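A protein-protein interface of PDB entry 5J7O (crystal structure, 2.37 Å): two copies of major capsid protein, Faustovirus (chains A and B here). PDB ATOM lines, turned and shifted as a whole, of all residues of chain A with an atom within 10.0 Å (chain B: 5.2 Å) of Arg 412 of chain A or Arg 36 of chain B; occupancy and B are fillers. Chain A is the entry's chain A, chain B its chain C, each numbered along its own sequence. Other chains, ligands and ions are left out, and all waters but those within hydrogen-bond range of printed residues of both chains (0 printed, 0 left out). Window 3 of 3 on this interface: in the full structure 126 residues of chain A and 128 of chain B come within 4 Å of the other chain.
Among the printed residues, merely in contact across the chains: Asp 407 of chain A with Thr 45 of chain B, Ile 408 of chain A with Pro 46 of chain B, Lys 411 of chain A with Thr 45 of chain B, Arg 412 of chain A with Arg 36 of chain B, Arg 412 of chain A with Leu 48 of chain B and Ile 413 of chain A with Leu 48 of chain B.
Arg 412 of chain A touches five residues of chain B.
Arg 36 of chain B touches one residue of chain A.
No residue of chain A comes within 4 Å of Leu 35 of chain B.
No residue of chain A comes within 4 Å of Ala 37 of chain B.
No residue of chain A comes within 4 Å of Gln 39 of chain B.
No residue of chain A comes within 4 Å of Gly 40 of chain B.
Phe 41 of chain B touches none of the printed residues of chain A.
Of chain A, only Ile 408 and Arg 412 come within 4 Å of Pro 46 of chain B.
Printed residues of chain A within 4 Å of Leu 48 of chain B: Arg 412 (3.9 Å) and Ile 413 (3.9 Å).
Printed residues of chain B within 4 Å of Lys 411 of chain A: Thr 45.
Of the printed residues of chain B, Ile 408 of chain A touches Pro 46.
The nearest residue of chain B that does not touch Arg 412 of chain A is Thr 47 of chain B (4.2 Å).
The nearest residue of chain A that does not touch Arg 36 of chain B is Ile 408 of chain A (9.1 Å).
The side-chain carboxylate of Asp 43 of chain B lies within salt-bridge range of the guanidinium group of Arg 412 of chain A (3.7 Å).
O of Pro 46 of chain B lies within hydrogen-bond range of NE of Arg 412 of chain A (3.1 Å).
O of Thr 45 of chain B sits at hydrogen-bond distance from NH2 of Arg 412 of chain A, 2.5 Å away.
No position is printed for both chains.
Of the 17 printed residues of chain B, 5 touch a printed residue of chain A.
Printed residues of chain B that touch a printed residue of chain A: Arg 36, Asp 43, Thr 45, Pro 46 and Leu 48.
Of the 15 printed residues of chain A, 5 touch a printed residue of chain B.
Hydrophobic or aromatic side chains of chain A within 4 Å of the printed part of chain B: Ile 408 and Ile 413.
Among the printed residues, Asp or Glu carboxylates within 4 Å of a Lys or Arg side-chain nitrogen of the other chain: Arg 412 of chain A with Asp 43 of chain B (3.7 Å).
OD2 of Asp 407 of chain A lies within salt-bridge range of NZ of Lys 411 of chain A (2.7 Å).
OD1 of Asp 43 of chain B is in hydrogen-bond range of OG1 of Thr 45 of chain B (2.6 Å).
The backbone NH (N) of Phe 41 of chain B lies within hydrogen-bond range of the backbone carbonyl oxygen (O) of Arg 36 of chain B, 3.1 Å away.
NH2 of Arg 36 of chain B lies within hydrogen-bond range of O of Asp 43 of chain B (2.6 Å).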
ATOM      1  N   GLU A 404     -19.843  22.219  -9.347  1.00  0.00           N
ATOM      2  CA  GLU A 404     -20.118  22.137 -10.778  1.00  0.00           C
ATOM      3  C   GLU A 404     -20.169  23.519 -11.418  1.00  0.00           C
ATOM      4  O   GLU A 404     -19.615  23.727 -12.504  1.00  0.00           O
ATOM      5  CB  GLU A 404     -21.430  21.387 -11.016  1.00  0.00           C
ATOM      6  CG  GLU A 404     -21.420  19.925 -10.584  1.00  0.00           C
ATOM      7  CD  GLU A 404     -21.616  19.739  -9.088  1.00  0.00           C
ATOM      8  OE1 GLU A 404     -21.602  20.746  -8.348  1.00  0.00           O
ATOM      9  OE2 GLU A 404     -21.787  18.581  -8.651  1.00  0.00           O
ATOM     10  N   ILE A 405     -20.828  24.475 -10.764  1.00  0.00           N
ATOM     11  CA  ILE A 405     -20.976  25.799 -11.357  1.00  0.00           C
ATOM     12  C   ILE A 405     -19.701  26.618 -11.175  1.00  0.00           C
ATOM     13  O   ILE A 405     -19.346  27.421 -12.047  1.00  0.00           O
ATOM     14  CB  ILE A 405     -22.213  26.512 -10.778  1.00  0.00           C
ATOM     15  CG1 ILE A 405     -23.499  25.977 -11.419  1.00  0.00           C
ATOM     16  CG2 ILE A 405     -22.137  28.018 -10.993  1.00  0.00           C
ATOM     17  CD1 ILE A 405     -23.906  24.589 -10.969  1.00  0.00           C
ATOM     18  N   HIS A 406     -18.983  26.417 -10.067  1.00  0.00           N
ATOM     19  CA  HIS A 406     -17.687  27.068  -9.900  1.00  0.00           C
ATOM     20  C   HIS A 406     -16.731  26.681 -11.020  1.00  0.00           C
ATOM     21  O   HIS A 406     -16.016  27.534 -11.559  1.00  0.00           O
ATOM     22  CB  HIS A 406     -17.085  26.710  -8.541  1.00  0.00           C
ATOM     23  CG  HIS A 406     -15.784  27.395  -8.257  1.00  0.00           C
ATOM     24  ND1 HIS A 406     -14.569  26.750  -8.339  1.00  0.00           N
ATOM     25  CD2 HIS A 406     -15.509  28.671  -7.897  1.00  0.00           C
ATOM     26  CE1 HIS A 406     -13.602  27.599  -8.038  1.00  0.00           C
ATOM     27  NE2 HIS A 406     -14.146  28.771  -7.766  1.00  0.00           N
ATOM     28  N   ASP A 407     -16.708  25.397 -11.384  1.00  0.00           N
ATOM     29  CA  ASP A 407     -15.851  24.941 -12.473  1.00  0.00           C
ATOM     30  C   ASP A 407     -16.206  25.640 -13.781  1.00  0.00           C
ATOM     31  O   ASP A 407     -15.329  26.174 -14.471  1.00  0.00           O
ATOM     32  CB  ASP A 407     -15.966  23.423 -12.620  1.00  0.00           C
ATOM     33  CG  ASP A 407     -15.179  22.887 -13.798  1.00  0.00           C
ATOM     34  OD1 ASP A 407     -15.761  22.758 -14.896  1.00  0.00           O
ATOM     35  OD2 ASP A 407     -13.978  22.594 -13.625  1.00  0.00           O
ATOM     36  N   ILE A 408     -17.492  25.649 -14.134  1.00  0.00           N
ATOM     37  CA  ILE A 408     -17.927  26.302 -15.367  1.00  0.00           C
ATOM     38  C   ILE A 408     -17.612  27.791 -15.323  1.00  0.00           C
ATOM     39  O   ILE A 408     -17.135  28.370 -16.308  1.00  0.00           O
ATOM     40  CB  ILE A 408     -19.428  26.053 -15.600  1.00  0.00           C
ATOM     41  CG1 ILE A 408     -19.702  24.564 -15.806  1.00  0.00           C
ATOM     42  CG2 ILE A 408     -19.927  26.866 -16.788  1.00  0.00           C
ATOM     43  CD1 ILE A 408     -21.170  24.232 -15.927  1.00  0.00           C
ATOM     44  N   TYR A 409     -17.864  28.432 -14.181  1.00  0.00           N
ATOM     45  CA  TYR A 409     -17.700  29.880 -14.091  1.00  0.00           C
ATOM     46  C   TYR A 409     -16.237  30.287 -14.214  1.00  0.00           C
ATOM     47  O   TYR A 409     -15.920  31.293 -14.857  1.00  0.00           O
ATOM     48  CB  TYR A 409     -18.293  30.392 -12.778  1.00  0.00           C
ATOM     49  CG  TYR A 409     -18.287  31.897 -12.650  1.00  0.00           C
ATOM     50  CD1 TYR A 409     -19.292  32.665 -13.222  1.00  0.00           C
ATOM     51  CD2 TYR A 409     -17.278  32.549 -11.955  1.00  0.00           C
ATOM     52  CE1 TYR A 409     -19.291  34.041 -13.107  1.00  0.00           C
ATOM     53  CE2 TYR A 409     -17.267  33.925 -11.835  1.00  0.00           C
ATOM     54  CZ  TYR A 409     -18.277  34.666 -12.413  1.00  0.00           C
ATOM     55  OH  TYR A 409     -18.273  36.036 -12.296  1.00  0.00           O
ATOM     56  N   ILE A 410     -15.330  29.519 -13.607  1.00  0.00           N
ATOM     57  CA  ILE A 410     -13.916  29.880 -13.647  1.00  0.00           C
ATOM     58  C   ILE A 410     -13.347  29.693 -15.049  1.00  0.00           C
ATOM     59  O   ILE A 410     -12.439  30.426 -15.463  1.00  0.00           O
ATOM     60  CB  ILE A 410     -13.142  29.071 -12.587  1.00  0.00           C
ATOM     61  CG1 ILE A 410     -13.536  29.537 -11.184  1.00  0.00           C
ATOM     62  CG2 ILE A 410     -11.640  29.201 -12.772  1.00  0.00           C
ATOM     63  CD1 ILE A 410     -13.371  31.028 -10.972  1.00  0.00           C
ATOM     64  N   LYS A 411     -13.887  28.744 -15.817  1.00  0.00           N
ATOM     65  CA  LYS A 411     -13.375  28.486 -17.157  1.00  0.00           C
ATOM     66  C   LYS A 411     -14.004  29.381 -18.221  1.00  0.00           C
ATOM     67  O   LYS A 411     -13.445  29.491 -19.318  1.00  0.00           O
ATOM     68  CB  LYS A 411     -13.601  27.019 -17.533  1.00  0.00           C
ATOM     69  CG  LYS A 411     -12.727  26.034 -16.770  1.00  0.00           C
ATOM     70  CD  LYS A 411     -13.174  24.599 -16.997  1.00  0.00           C
ATOM     71  CE  LYS A 411     -12.286  23.630 -16.234  1.00  0.00           C
ATOM     72  NZ  LYS A 411     -12.899  22.281 -16.105  1.00  0.00           N
ATOM     73  N   ARG A 412     -15.134  30.026 -17.929  1.00  0.00           N
ATOM     74  CA  ARG A 412     -15.903  30.713 -18.957  1.00  0.00           C
ATOM     75  C   ARG A 412     -16.113  32.202 -18.720  1.00  0.00           C
ATOM     76  O   ARG A 412     -16.577  32.887 -19.638  1.00  0.00           O
ATOM     77  CB  ARG A 412     -17.281  30.052 -19.122  1.00  0.00           C
ATOM     78  CG  ARG A 412     -17.245  28.604 -19.577  1.00  0.00           C
ATOM     79  CD  ARG A 412     -16.679  28.467 -20.980  1.00  0.00           C
ATOM     80  NE  ARG A 412     -16.945  27.146 -21.543  1.00  0.00           N
ATOM     81  CZ  ARG A 412     -16.513  26.737 -22.731  1.00  0.00           C
ATOM     82  NH1 ARG A 412     -15.787  27.546 -23.490  1.00  0.00           N
ATOM     83  NH2 ARG A 412     -16.807  25.518 -23.161  1.00  0.00           N
ATOM     84  N   ILE A 413     -15.802  32.727 -17.534  1.00  0.00           N
ATOM     85  CA  ILE A 413     -16.102  34.135 -17.284  1.00  0.00           C
ATOM     86  C   ILE A 413     -15.101  35.051 -17.989  1.00  0.00           C
ATOM     87  O   ILE A 413     -15.468  36.142 -18.442  1.00  0.00           O
ATOM     88  CB  ILE A 413     -16.167  34.416 -15.770  1.00  0.00           C
ATOM     89  CG1 ILE A 413     -16.726  35.817 -15.509  1.00  0.00           C
ATOM     90  CG2 ILE A 413     -14.806  34.259 -15.126  1.00  0.00           C
ATOM     91  CD1 ILE A 413     -18.163  35.991 -15.949  1.00  0.00           C
ATOM     92  N   GLY A 414     -13.842  34.636 -18.105  1.00  0.00           N
ATOM     93  CA  GLY A 414     -12.842  35.438 -18.787  1.00  0.00           C
ATOM     94  C   GLY A 414     -12.248  36.542 -17.937  1.00  0.00           C
ATOM     95  O   GLY A 414     -11.091  36.458 -17.512  1.00  0.00           O
ATOM     96  N   PHE A 415     -13.033  37.584 -17.675  1.00  0.00           N
ATOM     97  CA  PHE A 415     -12.556  38.734 -16.923  1.00  0.00           C
ATOM     98  C   PHE A 415     -13.728  39.380 -16.199  1.00  0.00           C
ATOM     99  O   PHE A 415     -14.888  39.003 -16.386  1.00  0.00           O
ATOM    100  CB  PHE A 415     -11.859  39.750 -17.835  1.00  0.00           C
ATOM    101  CG  PHE A 415     -12.780  40.407 -18.826  1.00  0.00           C
ATOM    102  CD1 PHE A 415     -13.128  39.762 -20.002  1.00  0.00           C
ATOM    103  CD2 PHE A 415     -13.292  41.672 -18.586  1.00  0.00           C
ATOM    104  CE1 PHE A 415     -13.974  40.363 -20.914  1.00  0.00           C
ATOM    105  CE2 PHE A 415     -14.136  42.279 -19.496  1.00  0.00           C
ATOM    106  CZ  PHE A 415     -14.476  41.623 -20.662  1.00  0.00           C
ATOM    107  N   THR A 416     -13.411  40.366 -15.364  1.00  0.00           N
ATOM    108  CA  THR A 416     -14.423  41.169 -14.692  1.00  0.00           C
ATOM    109  C   THR A 416     -14.025  42.633 -14.766  1.00  0.00           C
ATOM    110  O   THR A 416     -12.872  42.982 -14.492  1.00  0.00           O
ATOM    111  CB  THR A 416     -14.610  40.744 -13.227  1.00  0.00           C
ATOM    112  OG1 THR A 416     -15.441  41.701 -12.555  1.00  0.00           O
ATOM    113  CG2 THR A 416     -13.273  40.641 -12.505  1.00  0.00           C
ATOM    114  N   ILE A 621      -9.123  36.177 -14.583  1.00  0.00           N
ATOM    115  CA  ILE A 621      -9.736  35.214 -13.674  1.00  0.00           C
ATOM    116  C   ILE A 621      -8.900  33.941 -13.608  1.00  0.00           C
ATOM    117  O   ILE A 621      -7.826  33.861 -14.215  1.00  0.00           O
ATOM    118  CB  ILE A 621     -11.188  34.922 -14.110  1.00  0.00           C
ATOM    119  CG1 ILE A 621     -12.082  34.682 -12.889  1.00  0.00           C
ATOM    120  CG2 ILE A 621     -11.248  33.779 -15.132  1.00  0.00           C
ATOM    121  CD1 ILE A 621     -12.388  35.948 -12.114  1.00  0.00           C
ATOM    122  N   SER A 622      -9.375  32.952 -12.846  1.00  0.00           N
ATOM    123  CA  SER A 622      -8.776  31.618 -12.763  1.00  0.00           C
ATOM    124  C   SER A 622      -7.386  31.643 -12.138  1.00  0.00           C
ATOM    125  O   SER A 622      -6.992  30.698 -11.455  1.00  0.00           O
ATOM    126  CB  SER A 622      -8.711  30.961 -14.148  1.00  0.00           C
ATOM    127  OG  SER A 622      -7.731  31.575 -14.968  1.00  0.00           O
ATOM    128  N   SER B  31     -25.701  16.343 -19.204  1.00  0.00           N
ATOM    129  CA  SER B  31     -26.180  16.206 -20.575  1.00  0.00           C
ATOM    130  C   SER B  31     -25.373  17.066 -21.538  1.00  0.00           C
ATOM    131  O   SER B  31     -25.000  16.609 -22.623  1.00  0.00           O
ATOM    132  CB  SER B  31     -27.663  16.570 -20.646  1.00  0.00           C
ATOM    133  OG  SER B  31     -28.074  16.779 -21.986  1.00  0.00           O
ATOM    134  N   ILE B  32     -25.089  18.313 -21.157  1.00  0.00           N
ATOM    135  CA  ILE B  32     -24.415  19.234 -22.068  1.00  0.00           C
ATOM    136  C   ILE B  32     -22.971  18.803 -22.300  1.00  0.00           C
ATOM    137  O   ILE B  32     -22.464  18.870 -23.426  1.00  0.00           O
ATOM    138  CB  ILE B  32     -24.509  20.673 -21.531  1.00  0.00           C
ATOM    139  CG1 ILE B  32     -25.927  21.214 -21.725  1.00  0.00           C
ATOM    140  CG2 ILE B  32     -23.497  21.575 -22.216  1.00  0.00           C
ATOM    141  CD1 ILE B  32     -26.143  22.591 -21.145  1.00  0.00           C
ATOM    142  N   MET B  33     -22.286  18.348 -21.247  1.00  0.00           N
ATOM    143  CA  MET B  33     -20.914  17.879 -21.421  1.00  0.00           C
ATOM    144  C   MET B  33     -20.856  16.605 -22.253  1.00  0.00           C
ATOM    145  O   MET B  33     -19.872  16.378 -22.967  1.00  0.00           O
ATOM    146  CB  MET B  33     -20.254  17.654 -20.060  1.00  0.00           C
ATOM    147  CG  MET B  33     -20.061  18.921 -19.245  1.00  0.00           C
ATOM    148  SD  MET B  33     -19.202  18.629 -17.686  1.00  0.00           S
ATOM    149  CE  MET B  33     -17.589  18.113 -18.273  1.00  0.00           C
ATOM    150  N   CYS B  34     -21.894  15.769 -22.181  1.00  0.00           N
ATOM    151  CA  CYS B  34     -21.900  14.529 -22.951  1.00  0.00           C
ATOM    152  C   CYS B  34     -22.158  14.795 -24.429  1.00  0.00           C
ATOM    153  O   CYS B  34     -21.564  14.142 -25.295  1.00  0.00           O
ATOM    154  CB  CYS B  34     -22.945  13.567 -22.387  1.00  0.00           C
ATOM    155  SG  CYS B  34     -23.043  11.978 -23.247  1.00  0.00           S
ATOM    156  N   LEU B  35     -23.041  15.748 -24.737  1.00  0.00           N
ATOM    157  CA  LEU B  35     -23.313  16.086 -26.130  1.00  0.00           C
ATOM    158  C   LEU B  35     -22.109  16.761 -26.776  1.00  0.00           C
ATOM    159  O   LEU B  35     -21.691  16.383 -27.877  1.00  0.00           O
ATOM    160  CB  LEU B  35     -24.546  16.986 -26.220  1.00  0.00           C
ATOM    161  CG  LEU B  35     -25.870  16.396 -25.731  1.00  0.00           C
ATOM    162  CD1 LEU B  35     -26.905  17.493 -25.549  1.00  0.00           C
ATOM    163  CD2 LEU B  35     -26.378  15.339 -26.698  1.00  0.00           C
ATOM    164  N   ARG B  36     -21.541  17.765 -26.103  1.00  0.00           N
ATOM    165  CA  ARG B  36     -20.367  18.451 -26.635  1.00  0.00           C
ATOM    166  C   ARG B  36     -19.216  17.481 -26.869  1.00  0.00           C
ATOM    167  O   ARG B  36     -18.469  17.616 -27.845  1.00  0.00           O
ATOM    168  CB  ARG B  36     -19.931  19.564 -25.683  1.00  0.00           C
ATOM    169  CG  ARG B  36     -20.888  20.738 -25.594  1.00  0.00           C
ATOM    170  CD  ARG B  36     -20.311  21.825 -24.703  1.00  0.00           C
ATOM    171  NE  ARG B  36     -18.949  22.171 -25.098  1.00  0.00           N
ATOM    172  CZ  ARG B  36     -18.644  23.140 -25.955  1.00  0.00           C
ATOM    173  NH1 ARG B  36     -19.606  23.867 -26.507  1.00  0.00           N
ATOM    174  NH2 ARG B  36     -17.376  23.385 -26.259  1.00  0.00           N
ATOM    175  N   ALA B  37     -19.061  16.494 -25.985  1.00  0.00           N
ATOM    176  CA  ALA B  37     -17.967  15.538 -26.129  1.00  0.00           C
ATOM    177  C   ALA B  37     -18.148  14.668 -27.367  1.00  0.00           C
ATOM    178  O   ALA B  37     -17.186  14.430 -28.108  1.00  0.00           O
ATOM    179  CB  ALA B  37     -17.856  14.672 -24.875  1.00  0.00           C
ATOM    180  N   LYS B  38     -19.367  14.186 -27.613  1.00  0.00           N
ATOM    181  CA  LYS B  38     -19.601  13.336 -28.776  1.00  0.00           C
ATOM    182  C   LYS B  38     -19.630  14.129 -30.075  1.00  0.00           C
ATOM    183  O   LYS B  38     -19.316  13.578 -31.136  1.00  0.00           O
ATOM    184  CB  LYS B  38     -20.906  12.553 -28.615  1.00  0.00           C
ATOM    185  CG  LYS B  38     -20.790  11.315 -27.738  1.00  0.00           C
ATOM    186  CD  LYS B  38     -21.179  10.047 -28.492  1.00  0.00           C
ATOM    187  CE  LYS B  38     -20.111   9.632 -29.496  1.00  0.00           C
ATOM    188  NZ  LYS B  38     -20.416   8.312 -30.119  1.00  0.00           N
ATOM    189  N   GLN B  39     -19.997  15.408 -30.022  1.00  0.00           N
ATOM    190  CA  GLN B  39     -20.030  16.232 -31.224  1.00  0.00           C
ATOM    191  C   GLN B  39     -18.649  16.698 -31.666  1.00  0.00           C
ATOM    192  O   GLN B  39     -18.543  17.377 -32.692  1.00  0.00           O
ATOM    193  CB  GLN B  39     -20.945  17.442 -31.011  1.00  0.00           C
ATOM    194  CG  GLN B  39     -22.423  17.084 -30.960  1.00  0.00           C
ATOM    195  CD  GLN B  39     -23.311  18.289 -30.724  1.00  0.00           C
ATOM    196  OE1 GLN B  39     -22.843  19.427 -30.710  1.00  0.00           O
ATOM    197  NE2 GLN B  39     -24.602  18.042 -30.536  1.00  0.00           N
ATOM    198  N   GLY B  40     -17.598  16.354 -30.930  1.00  0.00           N
ATOM    199  CA  GLY B  40     -16.246  16.642 -31.354  1.00  0.00           C
ATOM    200  C   GLY B  40     -15.613  17.881 -30.763  1.00  0.00           C
ATOM    201  O   GLY B  40     -14.508  18.243 -31.182  1.00  0.00           O
ATOM    202  N   PHE B  41     -16.270  18.547 -29.818  1.00  0.00           N
ATOM    203  CA  PHE B  41     -15.647  19.679 -29.149  1.00  0.00           C
ATOM    204  C   PHE B  41     -14.493  19.203 -28.274  1.00  0.00           C
ATOM    205  O   PHE B  41     -14.523  18.110 -27.704  1.00  0.00           O
ATOM    206  CB  PHE B  41     -16.665  20.434 -28.295  1.00  0.00           C
ATOM    207  CG  PHE B  41     -17.718  21.155 -29.090  1.00  0.00           C
ATOM    208  CD1 PHE B  41     -17.485  22.431 -29.578  1.00  0.00           C
ATOM    209  CD2 PHE B  41     -18.945  20.562 -29.336  1.00  0.00           C
ATOM    210  CE1 PHE B  41     -18.455  23.098 -30.303  1.00  0.00           C
ATOM    211  CE2 PHE B  41     -19.917  21.224 -30.061  1.00  0.00           C
ATOM    212  CZ  PHE B  41     -19.672  22.493 -30.545  1.00  0.00           C
ATOM    213  N   ASP B  43     -13.324  21.175 -25.635  1.00  0.00           N
ATOM    214  CA  ASP B  43     -13.695  21.606 -24.296  1.00  0.00           C
ATOM    215  C   ASP B  43     -15.160  21.264 -24.062  1.00  0.00           C
ATOM    216  O   ASP B  43     -16.045  21.956 -24.590  1.00  0.00           O
ATOM    217  CB  ASP B  43     -13.458  23.110 -24.131  1.00  0.00           C
ATOM    218  CG  ASP B  43     -13.551  23.560 -22.685  1.00  0.00           C
ATOM    219  OD1 ASP B  43     -13.939  22.744 -21.822  1.00  0.00           O
ATOM    220  OD2 ASP B  43     -13.240  24.738 -22.411  1.00  0.00           O
ATOM    221  N   PRO B  44     -15.477  20.220 -23.290  1.00  0.00           N
ATOM    222  CA  PRO B  44     -16.885  19.863 -23.071  1.00  0.00           C
ATOM    223  C   PRO B  44     -17.587  20.703 -22.017  1.00  0.00           C
ATOM    224  O   PRO B  44     -18.807  20.557 -21.855  1.00  0.00           O
ATOM    225  CB  PRO B  44     -16.799  18.397 -22.629  1.00  0.00           C
ATOM    226  CG  PRO B  44     -15.485  18.315 -21.928  1.00  0.00           C
ATOM    227  CD  PRO B  44     -14.556  19.256 -22.661  1.00  0.00           C
ATOM    228  N   THR B  45     -16.871  21.564 -21.300  1.00  0.00           N
ATOM    229  CA  THR B  45     -17.500  22.343 -20.242  1.00  0.00           C
ATOM    230  C   THR B  45     -18.510  23.324 -20.836  1.00  0.00           C
ATOM    231  O   THR B  45     -18.225  23.980 -21.843  1.00  0.00           O
ATOM    232  CB  THR B  45     -16.453  23.097 -19.423  1.00  0.00           C
ATOM    233  OG1 THR B  45     -15.707  23.971 -20.277  1.00  0.00           O
ATOM    234  CG2 THR B  45     -15.504  22.118 -18.745  1.00  0.00           C
ATOM    235  N   PRO B  46     -19.694  23.440 -20.240  1.00  0.00           N
ATOM    236  CA  PRO B  46     -20.758  24.248 -20.844  1.00  0.00           C
ATOM    237  C   PRO B  46     -20.426  25.732 -20.855  1.00  0.00           C
ATOM    238  O   PRO B  46     -19.533  26.212 -20.153  1.00  0.00           O
ATOM    239  CB  PRO B  46     -21.971  23.967 -19.949  1.00  0.00           C
ATOM    240  CG  PRO B  46     -21.643  22.688 -19.238  1.00  0.00           C
ATOM    241  CD  PRO B  46     -20.160  22.706 -19.053  1.00  0.00           C
ATOM    242  N   THR B  47     -21.174  26.461 -21.677  1.00  0.00           N
ATOM    243  CA  THR B  47     -21.085  27.911 -21.736  1.00  0.00           C
ATOM    244  C   THR B  47     -22.004  28.525 -20.690  1.00  0.00           C
ATOM    245  O   THR B  47     -22.998  27.921 -20.280  1.00  0.00           O
ATOM    246  CB  THR B  47     -21.468  28.426 -23.125  1.00  0.00           C
ATOM    247  OG1 THR B  47     -22.895  28.459 -23.248  1.00  0.00           O
ATOM    248  CG2 THR B  47     -20.901  27.514 -24.202  1.00  0.00           C
ATOM    249  N   LEU B  48     -21.663  29.742 -20.257  1.00  0.00           N
ATOM    250  CA  LEU B  48     -22.478  30.411 -19.249  1.00  0.00           C
ATOM    251  C   LEU B  48     -23.896  30.663 -19.747  1.00  0.00           C
ATOM    252  O   LEU B  48     -24.830  30.738 -18.941  1.00  0.00           O
ATOM    253  CB  LEU B  48     -21.820  31.723 -18.819  1.00  0.00           C
ATOM    254  CG  LEU B  48     -20.600  31.581 -17.905  1.00  0.00           C
ATOM    255  CD1 LEU B  48     -20.058  32.946 -17.510  1.00  0.00           C
ATOM    256  CD2 LEU B  48     -20.950  30.760 -16.671  1.00  0.00           C
